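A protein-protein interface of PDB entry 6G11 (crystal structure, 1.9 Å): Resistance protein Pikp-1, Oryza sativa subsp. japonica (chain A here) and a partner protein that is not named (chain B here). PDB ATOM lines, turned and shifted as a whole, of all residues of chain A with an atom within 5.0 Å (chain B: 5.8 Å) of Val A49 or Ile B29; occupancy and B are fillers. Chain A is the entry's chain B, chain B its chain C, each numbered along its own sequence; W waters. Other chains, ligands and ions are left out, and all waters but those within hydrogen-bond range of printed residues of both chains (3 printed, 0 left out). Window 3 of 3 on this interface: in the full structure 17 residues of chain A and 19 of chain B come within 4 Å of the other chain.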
ATOM      1  N   LYS A   5     -27.069 -23.153  16.932  1.00  0.00           N
ATOM      2  CA  LYS A   5     -27.720 -22.090  16.069  1.00  0.00           C
ATOM      3  C   LYS A   5     -26.808 -21.304  15.085  1.00  0.00           C
ATOM      4  O   LYS A   5     -25.661 -20.892  15.415  1.00  0.00           O
ATOM      5  CB  LYS A   5     -28.529 -21.081  16.928  1.00  0.00           C
ATOM      6  CG  LYS A   5     -29.769 -21.594  17.702  1.00  0.00           C
ATOM      7  CD  LYS A   5     -30.680 -22.516  16.918  1.00  0.00           C
ATOM      8  CE  LYS A   5     -31.601 -23.350  17.787  1.00  0.00           C
ATOM      9  NZ  LYS A   5     -32.657 -22.566  18.445  1.00  0.00           N
ATOM     10  N   GLN A   6     -27.381 -20.982  13.927  1.00  0.00           N
ATOM     11  CA  GLN A   6     -26.781 -20.151  12.936  1.00  0.00           C
ATOM     12  C   GLN A   6     -27.233 -18.671  13.025  1.00  0.00           C
ATOM     13  O   GLN A   6     -28.353 -18.388  13.518  1.00  0.00           O
ATOM     14  CB  GLN A   6     -27.257 -20.625  11.568  1.00  0.00           C
ATOM     15  CG  GLN A   6     -27.120 -22.097  11.249  1.00  0.00           C
ATOM     16  CD  GLN A   6     -28.036 -22.449  10.076  1.00  0.00           C
ATOM     17  OE1 GLN A   6     -29.230 -22.603  10.246  1.00  0.00           O
ATOM     18  NE2 GLN A   6     -27.455 -22.553   8.847  1.00  0.00           N
ATOM     19  N   LYS A   7     -26.380 -17.771  12.551  1.00  0.00           N
ATOM     20  CA  LYS A   7     -26.738 -16.376  12.359  1.00  0.00           C
ATOM     21  C   LYS A   7     -26.335 -16.004  10.951  1.00  0.00           C
ATOM     22  O   LYS A   7     -25.166 -16.205  10.545  1.00  0.00           O
ATOM     23  CB  LYS A   7     -26.023 -15.440  13.339  1.00  0.00           C
ATOM     24  CG  LYS A   7     -26.421 -13.951  13.174  1.00  0.00           C
ATOM     25  CD  LYS A   7     -25.486 -13.005  13.921  1.00  0.00           C
ATOM     26  CE  LYS A   7     -25.549 -13.196  15.393  1.00  0.00           C
ATOM     27  NZ  LYS A   7     -24.447 -12.405  16.063  1.00  0.00           N
ATOM     28  N   GLY A  32     -36.915 -23.596  10.311  1.00  0.00           N
ATOM     29  CA  GLY A  32     -35.812 -23.457  11.284  1.00  0.00           C
ATOM     30  C   GLY A  32     -35.549 -22.062  11.840  1.00  0.00           C
ATOM     31  O   GLY A  32     -34.656 -21.871  12.640  1.00  0.00           O
ATOM     32  N   VAL A  33     -36.318 -21.067  11.385  1.00  0.00           N
ATOM     33  CA  VAL A  33     -36.110 -19.663  11.826  1.00  0.00           C
ATOM     34  C   VAL A  33     -36.589 -19.443  13.259  1.00  0.00           C
ATOM     35  O   VAL A  33     -37.731 -19.749  13.605  1.00  0.00           O
ATOM     36  CB  VAL A  33     -36.753 -18.694  10.846  1.00  0.00           C
ATOM     37  CG1 VAL A  33     -36.798 -17.262  11.388  1.00  0.00           C
ATOM     38  CG2 VAL A  33     -35.978 -18.763   9.564  1.00  0.00           C
ATOM     39  N   ASP A  34     -35.712 -18.911  14.088  1.00  0.00           N
ATOM     40  CA  ASP A  34     -36.067 -18.451  15.448  1.00  0.00           C
ATOM     41  C   ASP A  34     -36.376 -16.943  15.467  1.00  0.00           C
ATOM     42  O   ASP A  34     -37.303 -16.544  16.182  1.00  0.00           O
ATOM     43  CB  ASP A  34     -34.944 -18.667  16.447  1.00  0.00           C
ATOM     44  CG  ASP A  34     -34.608 -20.141  16.707  1.00  0.00           C
ATOM     45  OD1 ASP A  34     -35.455 -21.003  16.435  1.00  0.00           O
ATOM     46  OD2 ASP A  34     -33.501 -20.416  17.248  1.00  0.00           O
ATOM     47  N   SER A  35     -35.623 -16.121  14.717  1.00  0.00           N
ATOM     48  CA  SER A  35     -35.890 -14.687  14.673  1.00  0.00           C
ATOM     49  C   SER A  35     -35.430 -14.059  13.390  1.00  0.00           C
ATOM     50  O   SER A  35     -34.473 -14.541  12.782  1.00  0.00           O
ATOM     51  CB  SER A  35     -35.195 -13.959  15.849  1.00  0.00           C
ATOM     52  OG  SER A  35     -33.759 -14.058  15.774  1.00  0.00           O
ATOM     53  N   GLU A  47     -31.131  -9.779   9.760  1.00  0.00           N
ATOM     54  CA  GLU A  47     -30.401 -10.703  10.600  1.00  0.00           C
ATOM     55  C   GLU A  47     -31.350 -11.833  11.012  1.00  0.00           C
ATOM     56  O   GLU A  47     -32.399 -11.568  11.616  1.00  0.00           O
ATOM     57  CB  GLU A  47     -29.815  -9.977  11.824  1.00  0.00           C
ATOM     58  CG  GLU A  47     -29.029 -10.924  12.697  1.00  0.00           C
ATOM     59  CD  GLU A  47     -28.280 -10.243  13.845  1.00  0.00           C
ATOM     60  OE1 GLU A  47     -28.411 -10.757  14.975  1.00  0.00           O
ATOM     61  OE2 GLU A  47     -27.585  -9.232  13.670  1.00  0.00           O
ATOM     62  N   VAL A  48     -30.992 -13.076  10.667  1.00  0.00           N
ATOM     63  CA  VAL A  48     -31.826 -14.248  10.875  1.00  0.00           C
ATOM     64  C   VAL A  48     -31.041 -15.196  11.737  1.00  0.00           C
ATOM     65  O   VAL A  48     -29.865 -15.474  11.449  1.00  0.00           O
ATOM     66  CB  VAL A  48     -32.403 -14.908   9.574  1.00  0.00           C
ATOM     67  CG1 VAL A  48     -31.391 -15.337   8.623  1.00  0.00           C
ATOM     68  CG2 VAL A  48     -33.378 -16.051   9.853  1.00  0.00           C
ATOM     69  N   VAL A  49     -31.691 -15.677  12.802  1.00  0.00           N
ATOM     70  CA  VAL A  49     -31.102 -16.671  13.722  1.00  0.00           C
ATOM     71  C   VAL A  49     -31.984 -17.914  13.658  1.00  0.00           C
ATOM     72  O   VAL A  49     -33.228 -17.828  13.638  1.00  0.00           O
ATOM     73  CB  VAL A  49     -30.971 -16.148  15.150  1.00  0.00           C
ATOM     74  CG1 VAL A  49     -30.506 -17.257  16.109  1.00  0.00           C
ATOM     75  CG2 VAL A  49     -30.006 -14.968  15.208  1.00  0.00           C
ATOM     76  N   GLY A  50     -31.350 -19.071  13.562  1.00  0.00           N
ATOM     77  CA  GLY A  50     -32.100 -20.311  13.480  1.00  0.00           C
ATOM     78  C   GLY A  50     -31.252 -21.542  13.306  1.00  0.00           C
ATOM     79  O   GLY A  50     -30.090 -21.523  13.610  1.00  0.00           O
ATOM     80  N   TYR A  51     -31.869 -22.621  12.829  1.00  0.00           N
ATOM     81  CA  TYR A  51     -31.206 -23.928  12.684  1.00  0.00           C
ATOM     82  C   TYR A  51     -31.609 -24.527  11.368  1.00  0.00           C
ATOM     83  O   TYR A  51     -32.787 -24.471  10.991  1.00  0.00           O
ATOM     84  CB  TYR A  51     -31.681 -24.883  13.773  1.00  0.00           C
ATOM     85  CG  TYR A  51     -31.187 -26.302  13.665  1.00  0.00           C
ATOM     86  CD1 TYR A  51     -29.930 -26.684  14.177  1.00  0.00           C
ATOM     87  CD2 TYR A  51     -31.981 -27.276  13.067  1.00  0.00           C
ATOM     88  CE1 TYR A  51     -29.488 -28.011  14.069  1.00  0.00           C
ATOM     89  CE2 TYR A  51     -31.541 -28.587  12.952  1.00  0.00           C
ATOM     90  CZ  TYR A  51     -30.313 -28.945  13.455  1.00  0.00           C
ATOM     91  OH  TYR A  51     -29.933 -30.260  13.331  1.00  0.00           O
ATOM     92  N   ILE A  53     -30.844 -23.724   8.337  1.00  0.00           N
ATOM     93  CA  ILE A  53     -31.210 -22.760   7.301  1.00  0.00           C
ATOM     94  C   ILE A  53     -30.127 -22.846   6.247  1.00  0.00           C
ATOM     95  O   ILE A  53     -28.956 -22.782   6.580  1.00  0.00           O
ATOM     96  CB  ILE A  53     -31.300 -21.326   7.857  1.00  0.00           C
ATOM     97  CG1 ILE A  53     -32.341 -21.219   8.993  1.00  0.00           C
ATOM     98  CG2 ILE A  53     -31.652 -20.352   6.732  1.00  0.00           C
ATOM     99  CD1 ILE A  53     -32.160 -20.011   9.900  1.00  0.00           C
ATOM    100  N   ASN A  78     -23.239 -20.130  17.134  1.00  0.00           N
ATOM    101  CA  ASN A  78     -22.995 -19.081  18.139  1.00  0.00           C
ATOM    102  C   ASN A  78     -22.051 -19.567  19.269  1.00  0.00           C
ATOM    103  O   ASN A  78     -21.974 -20.776  19.557  1.00  0.00           O
ATOM    104  CB  ASN A  78     -24.301 -18.648  18.791  1.00  0.00           C
ATOM    105  CG  ASN A  78     -24.921 -19.767  19.583  1.00  0.00           C
ATOM    106  OD1 ASN A  78     -25.523 -20.664  19.007  1.00  0.00           O
ATOM    107  ND2 ASN A  78     -24.700 -19.781  20.900  1.00  0.00           N
ATOM    108  N   ASN B  26     -31.045 -11.753  19.798  1.00  0.00           N
ATOM    109  CA  ASN B  26     -32.001 -12.852  19.815  1.00  0.00           C
ATOM    110  C   ASN B  26     -32.102 -13.317  21.293  1.00  0.00           C
ATOM    111  O   ASN B  26     -31.064 -13.601  21.927  1.00  0.00           O
ATOM    112  CB  ASN B  26     -31.566 -13.992  18.895  1.00  0.00           C
ATOM    113  CG  ASN B  26     -32.445 -15.239  19.036  1.00  0.00           C
ATOM    114  OD1 ASN B  26     -32.222 -16.079  19.918  1.00  0.00           O
ATOM    115  ND2 ASN B  26     -33.450 -15.363  18.168  1.00  0.00           N
ATOM    116  N   PRO B  27     -33.329 -13.391  21.837  1.00  0.00           N
ATOM    117  CA  PRO B  27     -33.495 -13.780  23.256  1.00  0.00           C
ATOM    118  C   PRO B  27     -33.183 -15.237  23.604  1.00  0.00           C
ATOM    119  O   PRO B  27     -33.040 -15.537  24.756  1.00  0.00           O
ATOM    120  CB  PRO B  27     -34.976 -13.463  23.543  1.00  0.00           C
ATOM    121  CG  PRO B  27     -35.642 -13.517  22.209  1.00  0.00           C
ATOM    122  CD  PRO B  27     -34.619 -13.084  21.182  1.00  0.00           C
ATOM    123  N   GLY B  28     -33.057 -16.136  22.645  1.00  0.00           N
ATOM    124  CA  GLY B  28     -32.717 -17.521  22.938  1.00  0.00           C
ATOM    125  C   GLY B  28     -31.246 -17.889  22.889  1.00  0.00           C
ATOM    126  O   GLY B  28     -30.911 -19.054  23.044  1.00  0.00           O
ATOM    127  N   ILE B  29     -30.357 -16.933  22.614  1.00  0.00           N
ATOM    128  CA  ILE B  29     -28.924 -17.221  22.625  1.00  0.00           C
ATOM    129  C   ILE B  29     -28.266 -16.122  23.435  1.00  0.00           C
ATOM    130  O   ILE B  29     -28.845 -15.079  23.617  1.00  0.00           O
ATOM    131  CB  ILE B  29     -28.322 -17.327  21.204  1.00  0.00           C
ATOM    132  CG1 ILE B  29     -28.591 -16.075  20.349  1.00  0.00           C
ATOM    133  CG2 ILE B  29     -28.891 -18.546  20.484  1.00  0.00           C
ATOM    134  CD1 ILE B  29     -27.941 -16.181  18.972  1.00  0.00           C
ATOM    135  N   PRO B  30     -27.048 -16.361  23.947  1.00  0.00           N
ATOM    136  CA  PRO B  30     -26.379 -15.294  24.693  1.00  0.00           C
ATOM    137  C   PRO B  30     -26.205 -13.967  23.909  1.00  0.00           C
ATOM    138  O   PRO B  30     -26.100 -13.971  22.659  1.00  0.00           O
ATOM    139  CB  PRO B  30     -24.993 -15.910  25.037  1.00  0.00           C
ATOM    140  CG  PRO B  30     -25.156 -17.376  24.900  1.00  0.00           C
ATOM    141  CD  PRO B  30     -26.177 -17.548  23.798  1.00  0.00           C
ATOM    142  N   VAL B  31     -26.167 -12.870  24.652  1.00  0.00           N
ATOM    143  CA  VAL B  31     -26.060 -11.546  24.107  1.00  0.00           C
ATOM    144  C   VAL B  31     -24.591 -11.353  23.644  1.00  0.00           C
ATOM    145  O   VAL B  31     -23.653 -11.576  24.415  1.00  0.00           O
ATOM    146  CB  VAL B  31     -26.504 -10.489  25.135  1.00  0.00           C
ATOM    147  CG1 VAL B  31     -26.299  -9.064  24.608  1.00  0.00           C
ATOM    148  CG2 VAL B  31     -27.982 -10.690  25.466  1.00  0.00           C
ATOM    149  N   TYR B  51     -19.741 -11.649  19.077  1.00  0.00           N
ATOM    150  CA  TYR B  51     -19.223 -12.197  20.339  1.00  0.00           C
ATOM    151  C   TYR B  51     -17.757 -11.887  20.544  1.00  0.00           C
ATOM    152  O   TYR B  51     -16.992 -11.820  19.577  1.00  0.00           O
ATOM    153  CB  TYR B  51     -19.404 -13.712  20.372  1.00  0.00           C
ATOM    154  CG  TYR B  51     -20.841 -14.135  20.464  1.00  0.00           C
ATOM    155  CD1 TYR B  51     -21.555 -13.956  21.645  1.00  0.00           C
ATOM    156  CD2 TYR B  51     -21.495 -14.736  19.359  1.00  0.00           C
ATOM    157  CE1 TYR B  51     -22.885 -14.348  21.752  1.00  0.00           C
ATOM    158  CE2 TYR B  51     -22.813 -15.132  19.440  1.00  0.00           C
ATOM    159  CZ  TYR B  51     -23.513 -14.935  20.626  1.00  0.00           C
ATOM    160  OH  TYR B  51     -24.824 -15.308  20.715  1.00  0.00           O
HETATM  161  O   HOH W   1     -32.318 -18.800  19.254  1.00  0.00           O
HETATM  162  O   HOH W   2     -25.590 -13.878  18.458  1.00  0.00           O
HETATM  163  O   HOH W   3     -35.838 -16.629  19.180  1.00  0.00           O
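Water W2 lies within hydrogen-bond range of OH of Tyr B51 and NZ of Lys A7.
Water W1 bridges the side-chain amide oxygen of Asn B26 (2.8 Å) and the side-chain carboxylate of Asp A34 (2.8 Å).
Water W3 bridges ND2 of Asn B26 (2.9 Å) and O of Asp A34 (3.3 Å).
N of Gly B28 lies within hydrogen-bond range of OD1 of Asn B26 (2.9 Å).
The side-chain amide oxygen (OD1) of Asn B26 is in hydrogen-bond range of the backbone NH (N) of Ile B29, at 3.4 Å.
The backbone carbonyl oxygen (O) of Pro B30 lies within hydrogen-bond range of the side-chain hydroxyl (OH) of Tyr B51.
The backbone carbonyl oxygen (O) of Lys A5 is in hydrogen-bond range of the backbone NH (N) of Asn A78 (3.1 Å).
The backbone NH (N) of Asp A34 lies within hydrogen-bond range of the backbone carbonyl oxygen (O) of Val A49 (2.7 Å).
The backbone carbonyl oxygen of Ser A35 lies within hydrogen-bond range of the backbone NH of Val A49, 3.0 Å away.
Hydrophobic or aromatic side chains of chain B within 4 Å of the printed part of chain A: Ile B29, Pro B30 and Tyr B51.
Along chain B the printed residues that touch a printed residue of chain A span positions 26 to 51.
Among the printed residues, no Asp or Glu carboxylate lies within 4 Å of a Lys or Arg side-chain nitrogen of the other chain.
Val A49 touches Asn B26.
Ile B29 touches Val A49 (CD1 to CG1, 3.99 Å).
Pro B30 touches Asn A78 (CD to ND2, 3.9 Å).
Tyr B51 touches Asn A78 (CE2 to CB, 3.9 Å).
The side-chain hydroxyl (OG) of Ser A35 sits at hydrogen-bond distance from the side-chain amide nitrogen (ND2) of Asn B26, at 2.7 Å.
Of the printed residues of chain B, Ser A35 touches Asn B26 (2.7 Å).
Glu A47 touches none of the printed residues of chain B.
Of the printed residues of chain B, Val A49 touches Asn B26 and Ile B29.
Ile A53 touches none of the printed residues of chain B.
Of the printed residues of chain B, Asn A78 touches Pro B30 (3.9 Å) and Tyr B51 (3.9 Å).
Of the printed residues of chain A, Asn B26 touches Ser A35 (2.7 Å) and Val A49 (3.98 Å).
Of the printed residues of chain A, Ile B29 touches Val A49.
Printed residues of chain A within 4 Å of Tyr B51: Asn A78.
The nearest printed residue of chain B that does not touch Val A49 is Gly B28 (6.8 Å).
The nearest printed residue of chain A that does not touch Ile B29 is Lys A5 (4.2 Å).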
